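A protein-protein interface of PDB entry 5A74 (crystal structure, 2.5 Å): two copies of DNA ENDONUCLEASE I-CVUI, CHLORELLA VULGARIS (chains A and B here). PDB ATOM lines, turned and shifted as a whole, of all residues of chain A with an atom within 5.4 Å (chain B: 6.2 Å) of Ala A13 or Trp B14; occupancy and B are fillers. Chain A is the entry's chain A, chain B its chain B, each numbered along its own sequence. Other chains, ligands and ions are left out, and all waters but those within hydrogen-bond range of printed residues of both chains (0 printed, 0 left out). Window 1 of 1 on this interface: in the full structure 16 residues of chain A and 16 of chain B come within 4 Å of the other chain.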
ATOM      1  N   ASP A   8      13.674  13.664  37.430  1.00  0.00           N
ATOM      2  CA  ASP A   8      12.405  12.966  37.628  1.00  0.00           C
ATOM      3  C   ASP A   8      11.504  13.143  36.412  1.00  0.00           C
ATOM      4  O   ASP A   8      10.796  12.215  36.007  1.00  0.00           O
ATOM      5  CB  ASP A   8      11.695  13.448  38.892  1.00  0.00           C
ATOM      6  CG  ASP A   8      12.309  12.882  40.161  1.00  0.00           C
ATOM      7  OD1 ASP A   8      13.436  12.347  40.100  1.00  0.00           O
ATOM      8  OD2 ASP A   8      11.663  12.979  41.226  1.00  0.00           O
ATOM      9  N   GLN A   9      11.544  14.334  35.821  1.00  0.00           N
ATOM     10  CA  GLN A   9      10.741  14.609  34.634  1.00  0.00           C
ATOM     11  C   GLN A   9      11.216  13.782  33.445  1.00  0.00           C
ATOM     12  O   GLN A   9      10.415  13.415  32.579  1.00  0.00           O
ATOM     13  CB  GLN A   9      10.734  16.105  34.301  1.00  0.00           C
ATOM     14  CG  GLN A   9      10.078  16.985  35.375  1.00  0.00           C
ATOM     15  CD  GLN A   9       8.751  16.424  35.892  1.00  0.00           C
ATOM     16  OE1 GLN A   9       7.793  16.266  35.133  1.00  0.00           O
ATOM     17  NE2 GLN A   9       8.697  16.122  37.192  1.00  0.00           N
ATOM     18  N   LEU A  10      12.514  13.484  33.403  1.00  0.00           N
ATOM     19  CA  LEU A  10      13.055  12.631  32.351  1.00  0.00           C
ATOM     20  C   LEU A  10      12.516  11.213  32.505  1.00  0.00           C
ATOM     21  O   LEU A  10      12.174  10.554  31.511  1.00  0.00           O
ATOM     22  CB  LEU A  10      14.586  12.631  32.369  1.00  0.00           C
ATOM     23  CG  LEU A  10      15.251  13.764  31.585  1.00  0.00           C
ATOM     24  CD1 LEU A  10      16.761  13.561  31.465  1.00  0.00           C
ATOM     25  CD2 LEU A  10      14.623  13.893  30.216  1.00  0.00           C
ATOM     26  N   LYS A  11      12.439  10.756  33.756  1.00  0.00           N
ATOM     27  CA  LYS A  11      11.845   9.464  34.071  1.00  0.00           C
ATOM     28  C   LYS A  11      10.384   9.378  33.599  1.00  0.00           C
ATOM     29  O   LYS A  11      10.027   8.460  32.852  1.00  0.00           O
ATOM     30  CB  LYS A  11      11.942   9.187  35.575  1.00  0.00           C
ATOM     31  CG  LYS A  11      13.338   8.796  36.051  1.00  0.00           C
ATOM     32  CD  LYS A  11      13.892   7.623  35.235  1.00  0.00           C
ATOM     33  CE  LYS A  11      15.264   7.149  35.731  1.00  0.00           C
ATOM     34  NZ  LYS A  11      15.187   5.893  36.546  1.00  0.00           N
ATOM     35  N   PHE A  12       9.549  10.334  34.017  1.00  0.00           N
ATOM     36  CA  PHE A  12       8.124  10.299  33.686  1.00  0.00           C
ATOM     37  C   PHE A  12       7.875  10.341  32.178  1.00  0.00           C
ATOM     38  O   PHE A  12       6.986   9.653  31.677  1.00  0.00           O
ATOM     39  CB  PHE A  12       7.365  11.444  34.374  1.00  0.00           C
ATOM     40  CG  PHE A  12       7.538  11.485  35.874  1.00  0.00           C
ATOM     41  CD1 PHE A  12       7.695  10.317  36.611  1.00  0.00           C
ATOM     42  CD2 PHE A  12       7.540  12.703  36.548  1.00  0.00           C
ATOM     43  CE1 PHE A  12       7.849  10.369  37.989  1.00  0.00           C
ATOM     44  CE2 PHE A  12       7.700  12.758  37.928  1.00  0.00           C
ATOM     45  CZ  PHE A  12       7.853  11.591  38.645  1.00  0.00           C
ATOM     46  N   ALA A  13       8.656  11.151  31.463  1.00  0.00           N
ATOM     47  CA  ALA A  13       8.559  11.246  29.997  1.00  0.00           C
ATOM     48  C   ALA A  13       8.825   9.890  29.327  1.00  0.00           C
ATOM     49  O   ALA A  13       8.095   9.480  28.407  1.00  0.00           O
ATOM     50  CB  ALA A  13       9.516  12.313  29.460  1.00  0.00           C
ATOM     51  N   TRP A  14       9.868   9.202  29.800  1.00  0.00           N
ATOM     52  CA  TRP A  14      10.168   7.843  29.363  1.00  0.00           C
ATOM     53  C   TRP A  14       9.031   6.884  29.726  1.00  0.00           C
ATOM     54  O   TRP A  14       8.632   6.044  28.909  1.00  0.00           O
ATOM     55  CB  TRP A  14      11.476   7.351  29.981  1.00  0.00           C
ATOM     56  CG  TRP A  14      11.731   5.894  29.712  1.00  0.00           C
ATOM     57  CD1 TRP A  14      12.395   5.357  28.642  1.00  0.00           C
ATOM     58  CD2 TRP A  14      11.321   4.783  30.525  1.00  0.00           C
ATOM     59  NE1 TRP A  14      12.417   3.984  28.741  1.00  0.00           N
ATOM     60  CE2 TRP A  14      11.760   3.609  29.888  1.00  0.00           C
ATOM     61  CE3 TRP A  14      10.615   4.671  31.726  1.00  0.00           C
ATOM     62  CZ2 TRP A  14      11.519   2.346  30.407  1.00  0.00           C
ATOM     63  CZ3 TRP A  14      10.379   3.420  32.240  1.00  0.00           C
ATOM     64  CH2 TRP A  14      10.833   2.271  31.585  1.00  0.00           C
ATOM     65  N   LEU A  15       8.514   7.001  30.949  1.00  0.00           N
ATOM     66  CA  LEU A  15       7.420   6.132  31.385  1.00  0.00           C
ATOM     67  C   LEU A  15       6.145   6.365  30.562  1.00  0.00           C
ATOM     68  O   LEU A  15       5.442   5.419  30.203  1.00  0.00           O
ATOM     69  CB  LEU A  15       7.148   6.299  32.884  1.00  0.00           C
ATOM     70  CG  LEU A  15       6.061   5.393  33.486  1.00  0.00           C
ATOM     71  CD1 LEU A  15       6.253   3.947  33.065  1.00  0.00           C
ATOM     72  CD2 LEU A  15       6.051   5.490  35.007  1.00  0.00           C
ATOM     73  N   ALA A  16       5.861   7.623  30.250  1.00  0.00           N
ATOM     74  CA  ALA A  16       4.686   7.956  29.456  1.00  0.00           C
ATOM     75  C   ALA A  16       4.766   7.260  28.104  1.00  0.00           C
ATOM     76  O   ALA A  16       3.775   6.689  27.622  1.00  0.00           O
ATOM     77  CB  ALA A  16       4.575   9.463  29.278  1.00  0.00           C
ATOM     78  N   GLY A  17       5.957   7.315  27.508  1.00  0.00           N
ATOM     79  CA  GLY A  17       6.232   6.626  26.261  1.00  0.00           C
ATOM     80  C   GLY A  17       5.910   5.155  26.405  1.00  0.00           C
ATOM     81  O   GLY A  17       5.143   4.604  25.602  1.00  0.00           O
ATOM     82  N   PHE A  18       6.473   4.531  27.443  1.00  0.00           N
ATOM     83  CA  PHE A  18       6.237   3.122  27.715  1.00  0.00           C
ATOM     84  C   PHE A  18       4.762   2.830  27.899  1.00  0.00           C
ATOM     85  O   PHE A  18       4.231   1.876  27.322  1.00  0.00           O
ATOM     86  CB  PHE A  18       6.996   2.683  28.954  1.00  0.00           C
ATOM     87  CG  PHE A  18       7.444   1.252  28.904  1.00  0.00           C
ATOM     88  CD1 PHE A  18       8.578   0.896  28.188  1.00  0.00           C
ATOM     89  CD2 PHE A  18       6.731   0.255  29.561  1.00  0.00           C
ATOM     90  CE1 PHE A  18       8.992  -0.433  28.135  1.00  0.00           C
ATOM     91  CE2 PHE A  18       7.148  -1.076  29.518  1.00  0.00           C
ATOM     92  CZ  PHE A  18       8.272  -1.420  28.811  1.00  0.00           C
ATOM     93  N   ASP A  20       2.215   4.766  26.883  1.00  0.00           N
ATOM     94  CA  ASP A  20       1.552   5.041  25.601  1.00  0.00           C
ATOM     95  C   ASP A  20       1.601   3.812  24.686  1.00  0.00           C
ATOM     96  O   ASP A  20       0.675   3.557  23.907  1.00  0.00           O
ATOM     97  CB  ASP A  20       2.168   6.259  24.894  1.00  0.00           C
ATOM     98  CG  ASP A  20       1.466   7.564  25.245  1.00  0.00           C
ATOM     99  OD1 ASP A  20       0.291   7.511  25.679  1.00  0.00           O
ATOM    100  OD2 ASP A  20       2.089   8.643  25.072  1.00  0.00           O
ATOM    101  N   TYR A  97       3.267  14.275  29.509  1.00  0.00           N
ATOM    102  CA  TYR A  97       4.037  13.552  28.496  1.00  0.00           C
ATOM    103  C   TYR A  97       3.256  12.468  27.737  1.00  0.00           C
ATOM    104  O   TYR A  97       3.713  11.977  26.704  1.00  0.00           O
ATOM    105  CB  TYR A  97       5.299  12.968  29.120  1.00  0.00           C
ATOM    106  CG  TYR A  97       6.021  13.929  30.037  1.00  0.00           C
ATOM    107  CD1 TYR A  97       6.754  14.994  29.526  1.00  0.00           C
ATOM    108  CD2 TYR A  97       5.971  13.769  31.414  1.00  0.00           C
ATOM    109  CE1 TYR A  97       7.416  15.870  30.365  1.00  0.00           C
ATOM    110  CE2 TYR A  97       6.630  14.639  32.260  1.00  0.00           C
ATOM    111  CZ  TYR A  97       7.350  15.684  31.731  1.00  0.00           C
ATOM    112  OH  TYR A  97       8.006  16.547  32.578  1.00  0.00           O
ATOM    113  N   LEU A  98       2.075  12.140  28.160  1.00  0.00           N
ATOM    114  CA  LEU A  98       1.275  11.172  27.456  1.00  0.00           C
ATOM    115  C   LEU A  98       0.779  11.662  26.089  1.00  0.00           C
ATOM    116  O   LEU A  98       0.211  12.698  25.971  1.00  0.00           O
ATOM    117  CB  LEU A  98       0.124  10.703  28.313  1.00  0.00           C
ATOM    118  CG  LEU A  98       0.421   9.837  29.517  1.00  0.00           C
ATOM    119  CD1 LEU A  98      -0.664   9.840  30.547  1.00  0.00           C
ATOM    120  CD2 LEU A  98       0.805   8.429  29.119  1.00  0.00           C
ATOM    121  N   GLN A  99       1.055  10.909  25.049  1.00  0.00           N
ATOM    122  CA  GLN A  99       0.603  11.248  23.727  1.00  0.00           C
ATOM    123  C   GLN A  99      -0.550  10.456  23.178  1.00  0.00           C
ATOM    124  O   GLN A  99      -1.231  10.936  22.377  1.00  0.00           O
ATOM    125  CB  GLN A  99       1.744  11.214  22.727  1.00  0.00           C
ATOM    126  CG  GLN A  99       2.995  11.883  23.179  1.00  0.00           C
ATOM    127  CD  GLN A  99       2.798  13.323  23.420  1.00  0.00           C
ATOM    128  OE1 GLN A  99       2.202  13.980  22.666  1.00  0.00           O
ATOM    129  NE2 GLN A  99       3.295  13.805  24.506  1.00  0.00           N
ATOM    130  N   GLN B   9      15.285  16.747  25.006  1.00  0.00           N
ATOM    131  CA  GLN B   9      15.645  15.596  25.821  1.00  0.00           C
ATOM    132  C   GLN B   9      14.393  14.901  26.350  1.00  0.00           C
ATOM    133  O   GLN B   9      14.389  13.687  26.545  1.00  0.00           O
ATOM    134  CB  GLN B   9      16.583  15.993  26.967  1.00  0.00           C
ATOM    135  CG  GLN B   9      17.944  16.521  26.508  1.00  0.00           C
ATOM    136  CD  GLN B   9      18.607  15.629  25.463  1.00  0.00           C
ATOM    137  OE1 GLN B   9      18.853  14.448  25.705  1.00  0.00           O
ATOM    138  NE2 GLN B   9      18.898  16.196  24.296  1.00  0.00           N
ATOM    139  N   LEU B  10      13.325  15.664  26.566  1.00  0.00           N
ATOM    140  CA  LEU B  10      12.078  15.073  27.042  1.00  0.00           C
ATOM    141  C   LEU B  10      11.417  14.292  25.916  1.00  0.00           C
ATOM    142  O   LEU B  10      10.874  13.204  26.132  1.00  0.00           O
ATOM    143  CB  LEU B  10      11.136  16.144  27.595  1.00  0.00           C
ATOM    144  CG  LEU B  10      11.578  16.802  28.902  1.00  0.00           C
ATOM    145  CD1 LEU B  10      10.649  17.953  29.280  1.00  0.00           C
ATOM    146  CD2 LEU B  10      11.618  15.785  30.010  1.00  0.00           C
ATOM    147  N   LYS B  11      11.473  14.858  24.713  1.00  0.00           N
ATOM    148  CA  LYS B  11      10.989  14.186  23.512  1.00  0.00           C
ATOM    149  C   LYS B  11      11.722  12.859  23.301  1.00  0.00           C
ATOM    150  O   LYS B  11      11.088  11.834  23.034  1.00  0.00           O
ATOM    151  CB  LYS B  11      11.159  15.093  22.287  1.00  0.00           C
ATOM    152  CG  LYS B  11      10.038  16.125  22.086  1.00  0.00           C
ATOM    153  CD  LYS B  11       8.704  15.433  21.800  1.00  0.00           C
ATOM    154  CE  LYS B  11       7.608  16.401  21.326  1.00  0.00           C
ATOM    155  NZ  LYS B  11       7.016  17.204  22.438  1.00  0.00           N
ATOM    156  N   PHE B  12      13.051  12.874  23.446  1.00  0.00           N
ATOM    157  CA  PHE B  12      13.849  11.664  23.246  1.00  0.00           C
ATOM    158  C   PHE B  12      13.577  10.617  24.329  1.00  0.00           C
ATOM    159  O   PHE B  12      13.488   9.423  24.031  1.00  0.00           O
ATOM    160  CB  PHE B  12      15.348  11.987  23.193  1.00  0.00           C
ATOM    161  CG  PHE B  12      15.729  12.934  22.097  1.00  0.00           C
ATOM    162  CD1 PHE B  12      15.008  12.980  20.905  1.00  0.00           C
ATOM    163  CD2 PHE B  12      16.820  13.783  22.251  1.00  0.00           C
ATOM    164  CE1 PHE B  12      15.371  13.863  19.885  1.00  0.00           C
ATOM    165  CE2 PHE B  12      17.188  14.669  21.239  1.00  0.00           C
ATOM    166  CZ  PHE B  12      16.461  14.708  20.056  1.00  0.00           C
ATOM    167  N   ALA B  13      13.454  11.059  25.578  1.00  0.00           N
ATOM    168  CA  ALA B  13      13.162  10.137  26.678  1.00  0.00           C
ATOM    169  C   ALA B  13      11.830   9.436  26.429  1.00  0.00           C
ATOM    170  O   ALA B  13      11.726   8.209  26.587  1.00  0.00           O
ATOM    171  CB  ALA B  13      13.153  10.865  28.024  1.00  0.00           C
ATOM    172  N   TRP B  14      10.825  10.210  26.013  1.00  0.00           N
ATOM    173  CA  TRP B  14       9.520   9.649  25.676  1.00  0.00           C
ATOM    174  C   TRP B  14       9.635   8.664  24.522  1.00  0.00           C
ATOM    175  O   TRP B  14       9.087   7.563  24.586  1.00  0.00           O
ATOM    176  CB  TRP B  14       8.515  10.744  25.318  1.00  0.00           C
ATOM    177  CG  TRP B  14       7.172  10.191  24.862  1.00  0.00           C
ATOM    178  CD1 TRP B  14       6.075   9.931  25.646  1.00  0.00           C
ATOM    179  CD2 TRP B  14       6.794   9.846  23.523  1.00  0.00           C
ATOM    180  NE1 TRP B  14       5.050   9.436  24.876  1.00  0.00           N
ATOM    181  CE2 TRP B  14       5.467   9.375  23.567  1.00  0.00           C
ATOM    182  CE3 TRP B  14       7.449   9.889  22.288  1.00  0.00           C
ATOM    183  CZ2 TRP B  14       4.786   8.948  22.424  1.00  0.00           C
ATOM    184  CZ3 TRP B  14       6.774   9.467  21.157  1.00  0.00           C
ATOM    185  CH2 TRP B  14       5.456   9.003  21.233  1.00  0.00           C
ATOM    186  N   LEU B  15      10.332   9.067  23.462  1.00  0.00           N
ATOM    187  CA  LEU B  15      10.484   8.199  22.297  1.00  0.00           C
ATOM    188  C   LEU B  15      11.170   6.896  22.683  1.00  0.00           C
ATOM    189  O   LEU B  15      10.773   5.823  22.222  1.00  0.00           O
ATOM    190  CB  LEU B  15      11.254   8.891  21.179  1.00  0.00           C
ATOM    191  CG  LEU B  15      11.440   8.009  19.943  1.00  0.00           C
ATOM    192  CD1 LEU B  15      10.113   7.444  19.448  1.00  0.00           C
ATOM    193  CD2 LEU B  15      12.116   8.798  18.852  1.00  0.00           C
ATOM    194  N   ALA B  16      12.182   6.991  23.537  1.00  0.00           N
ATOM    195  CA  ALA B  16      12.857   5.800  24.035  1.00  0.00           C
ATOM    196  C   ALA B  16      11.866   4.848  24.723  1.00  0.00           C
ATOM    197  O   ALA B  16      11.884   3.628  24.471  1.00  0.00           O
ATOM    198  CB  ALA B  16      13.986   6.184  24.971  1.00  0.00           C
ATOM    199  N   GLY B  17      11.006   5.402  25.578  1.00  0.00           N
ATOM    200  CA  GLY B  17       9.978   4.604  26.226  1.00  0.00           C
ATOM    201  C   GLY B  17       9.152   3.895  25.169  1.00  0.00           C
ATOM    202  O   GLY B  17       9.039   2.666  25.161  1.00  0.00           O
ATOM    203  N   PHE B  18       8.623   4.676  24.237  1.00  0.00           N
ATOM    204  CA  PHE B  18       7.833   4.120  23.152  1.00  0.00           C
ATOM    205  C   PHE B  18       8.604   3.071  22.346  1.00  0.00           C
ATOM    206  O   PHE B  18       8.035   2.060  21.927  1.00  0.00           O
ATOM    207  CB  PHE B  18       7.336   5.230  22.234  1.00  0.00           C
ATOM    208  CG  PHE B  18       6.022   4.918  21.595  1.00  0.00           C
ATOM    209  CD1 PHE B  18       5.966   4.244  20.385  1.00  0.00           C
ATOM    210  CD2 PHE B  18       4.838   5.266  22.222  1.00  0.00           C
ATOM    211  CE1 PHE B  18       4.748   3.943  19.805  1.00  0.00           C
ATOM    212  CE2 PHE B  18       3.619   4.962  21.650  1.00  0.00           C
ATOM    213  CZ  PHE B  18       3.576   4.301  20.445  1.00  0.00           C
ATOM    214  N   VAL B  19       9.895   3.309  22.134  1.00  0.00           N
ATOM    215  CA  VAL B  19      10.727   2.326  21.446  1.00  0.00           C
ATOM    216  C   VAL B  19      10.949   1.101  22.338  1.00  0.00           C
ATOM    217  O   VAL B  19      10.812  -0.040  21.868  1.00  0.00           O
ATOM    218  CB  VAL B  19      12.077   2.920  20.932  1.00  0.00           C
ATOM    219  CG1 VAL B  19      13.010   1.823  20.421  1.00  0.00           C
ATOM    220  CG2 VAL B  19      11.817   3.918  19.824  1.00  0.00           C
ATOM    221  N   ILE B  56       0.899   9.270  15.212  1.00  0.00           N
ATOM    222  CA  ILE B  56       2.027   9.270  16.142  1.00  0.00           C
ATOM    223  C   ILE B  56       3.364   8.937  15.446  1.00  0.00           C
ATOM    224  O   ILE B  56       4.424   9.435  15.843  1.00  0.00           O
ATOM    225  CB  ILE B  56       1.767   8.324  17.346  1.00  0.00           C
ATOM    226  CG1 ILE B  56       2.703   8.646  18.516  1.00  0.00           C
ATOM    227  CG2 ILE B  56       1.884   6.860  16.940  1.00  0.00           C
ATOM    228  CD1 ILE B  56       2.305   9.909  19.259  1.00  0.00           C
ATOM    229  N   ILE B  60       6.857  11.060  15.300  1.00  0.00           N
ATOM    230  CA  ILE B  60       8.207  10.566  15.571  1.00  0.00           C
ATOM    231  C   ILE B  60       9.173  10.998  14.474  1.00  0.00           C
ATOM    232  O   ILE B  60      10.267  11.481  14.754  1.00  0.00           O
ATOM    233  CB  ILE B  60       8.206   9.042  15.753  1.00  0.00           C
ATOM    234  CG1 ILE B  60       7.472   8.698  17.058  1.00  0.00           C
ATOM    235  CG2 ILE B  60       9.626   8.499  15.761  1.00  0.00           C
ATOM    236  CD1 ILE B  60       7.064   7.252  17.190  1.00  0.00           C
ATOM    237  N   ILE B  63      10.078  14.471  15.125  1.00  0.00           N
ATOM    238  CA  ILE B  63      11.018  14.512  16.243  1.00  0.00           C
ATOM    239  C   ILE B  63      12.472  14.174  15.844  1.00  0.00           C
ATOM    240  O   ILE B  63      13.406  14.870  16.257  1.00  0.00           O
ATOM    241  CB  ILE B  63      10.565  13.555  17.349  1.00  0.00           C
ATOM    242  CG1 ILE B  63       9.274  14.056  17.999  1.00  0.00           C
ATOM    243  CG2 ILE B  63      11.653  13.373  18.403  1.00  0.00           C
ATOM    244  CD1 ILE B  63       8.702  13.084  19.030  1.00  0.00           C
ATOM    245  N   TYR B  97      18.494   7.089  27.227  1.00  0.00           N
ATOM    246  CA  TYR B  97      17.174   6.849  27.806  1.00  0.00           C
ATOM    247  C   TYR B  97      16.618   5.428  27.589  1.00  0.00           C
ATOM    248  O   TYR B  97      15.721   4.999  28.311  1.00  0.00           O
ATOM    249  CB  TYR B  97      16.179   7.915  27.332  1.00  0.00           C
ATOM    250  CG  TYR B  97      16.709   9.337  27.423  1.00  0.00           C
ATOM    251  CD1 TYR B  97      16.913   9.950  28.653  1.00  0.00           C
ATOM    252  CD2 TYR B  97      16.993  10.065  26.275  1.00  0.00           C
ATOM    253  CE1 TYR B  97      17.393  11.246  28.737  1.00  0.00           C
ATOM    254  CE2 TYR B  97      17.471  11.360  26.349  1.00  0.00           C
ATOM    255  CZ  TYR B  97      17.667  11.945  27.581  1.00  0.00           C
ATOM    256  OH  TYR B  97      18.146  13.234  27.653  1.00  0.00           O
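The side-chain amide oxygen of Gln A9 lies within hydrogen-bond range of the side-chain hydroxyl of Tyr A97 (2.6 Å). The backbone NH (N) of Gln A99 is in hydrogen-bond range of the side-chain carboxylate (OD2) of Asp A20 (2.5 Å). The backbone carbonyl oxygen of Tyr A97 lies within hydrogen-bond range of the side-chain amide nitrogen of Gln A99 (2.9 Å). OE1 of Gln B9 sits at hydrogen-bond distance from OH of Tyr B97 (2.4 Å).
Hydrophobic or aromatic side chains of chain B that line the printed part of chain A: Leu B10, Ala B13, Trp B14, Phe B18, Ile B56 and Tyr B97. Hydrophobic or aromatic side chains of chain A within 4 Å of the printed part of chain B: Leu A10, Ala A13, Trp A14, Ala A16, Phe A18 and Tyr A97. Among the printed residues, no Asp or Glu carboxylate lies within 4 Å of a Lys or Arg side-chain nitrogen of the other chain.
Among the printed residues, pairs that only touch across the chains: Ala A13 with Trp B14 (3.1 Å), Trp A14 with Ala B13 (3.2 Å), Trp A14 with Gly B17 (3.3 Å), Gly A17 with Phe B18 (3.5 Å), Gln A99 with Trp B14 (3.5 Å), Phe A18 with Gly B17 (3.5 Å), Leu A10 with Leu B10 (3.6 Å), Leu A10 with Tyr B97 (3.6 Å), Leu A10 with Ala B13 (3.6 Å), Leu A10 with Gln B9 (3.7 Å), Gly A17 with Gly B17 (3.7 Å), Gln A9 with Leu B10 (3.7 Å), Ala A13 with Leu B10 (3.7 Å), Gln A99 with Ile B56 (3.7 Å), Asp A20 with Phe B18 (3.8 Å), Ala A16 with Trp B14 (3.9 Å), Phe A18 with Phe B18 (3.9 Å), Trp A14 with Ala B16 (3.99 Å) and Tyr A97 with Leu B10 (3.996 Å).
Ala A13 touches two residues of chain B. Printed residues of chain A within 4 Å of Gln B9: Leu A10 (3.7 Å). Of the printed residues of chain A, Ala B13 touches Leu A10 (3.6 Å) and Trp A14 (3.2 Å). Printed residues of chain B within 4 Å of Gly A17: Trp B14, Gly B17 and Phe B18. Ile B60 touches none of the printed residues of chain A. Phe B12 touches none of the printed residues of chain A.
The indole nitrogen (NE1) of Trp A14 lies close to the backbone carbonyl oxygen (O) of Tyr B97 (3.5 Å). The side-chain carboxylate (OD2) of Asp A20 lies within hydrogen-bond range of the indole nitrogen (NE1) of Trp B14 (3.1 Å). O of Tyr A97 sits close to NE1 of Trp B14 (3.4 Å). N of Gly A17 sits close to NE1 of Trp B14, 3.5 Å away.
Gln A9 touches Leu B10, and with the chains exchanged Leu A10 touches Gln B9. Leu A10 touches Tyr B97, and with the chains exchanged Tyr A97 touches Leu B10. Ala A13 touches Trp B14, and with the chains exchanged Trp A14 touches Ala B13. Gly B17 touches its own counterpart, Gly A17. Positions printed for both chains: 9, 10, 11, 12, 13, 14, 15, 16, 17, 18 and 97. Of the 23 pairs that touch across the chains among the printed residues, 19 have their exchanged pair printed and touching as well.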
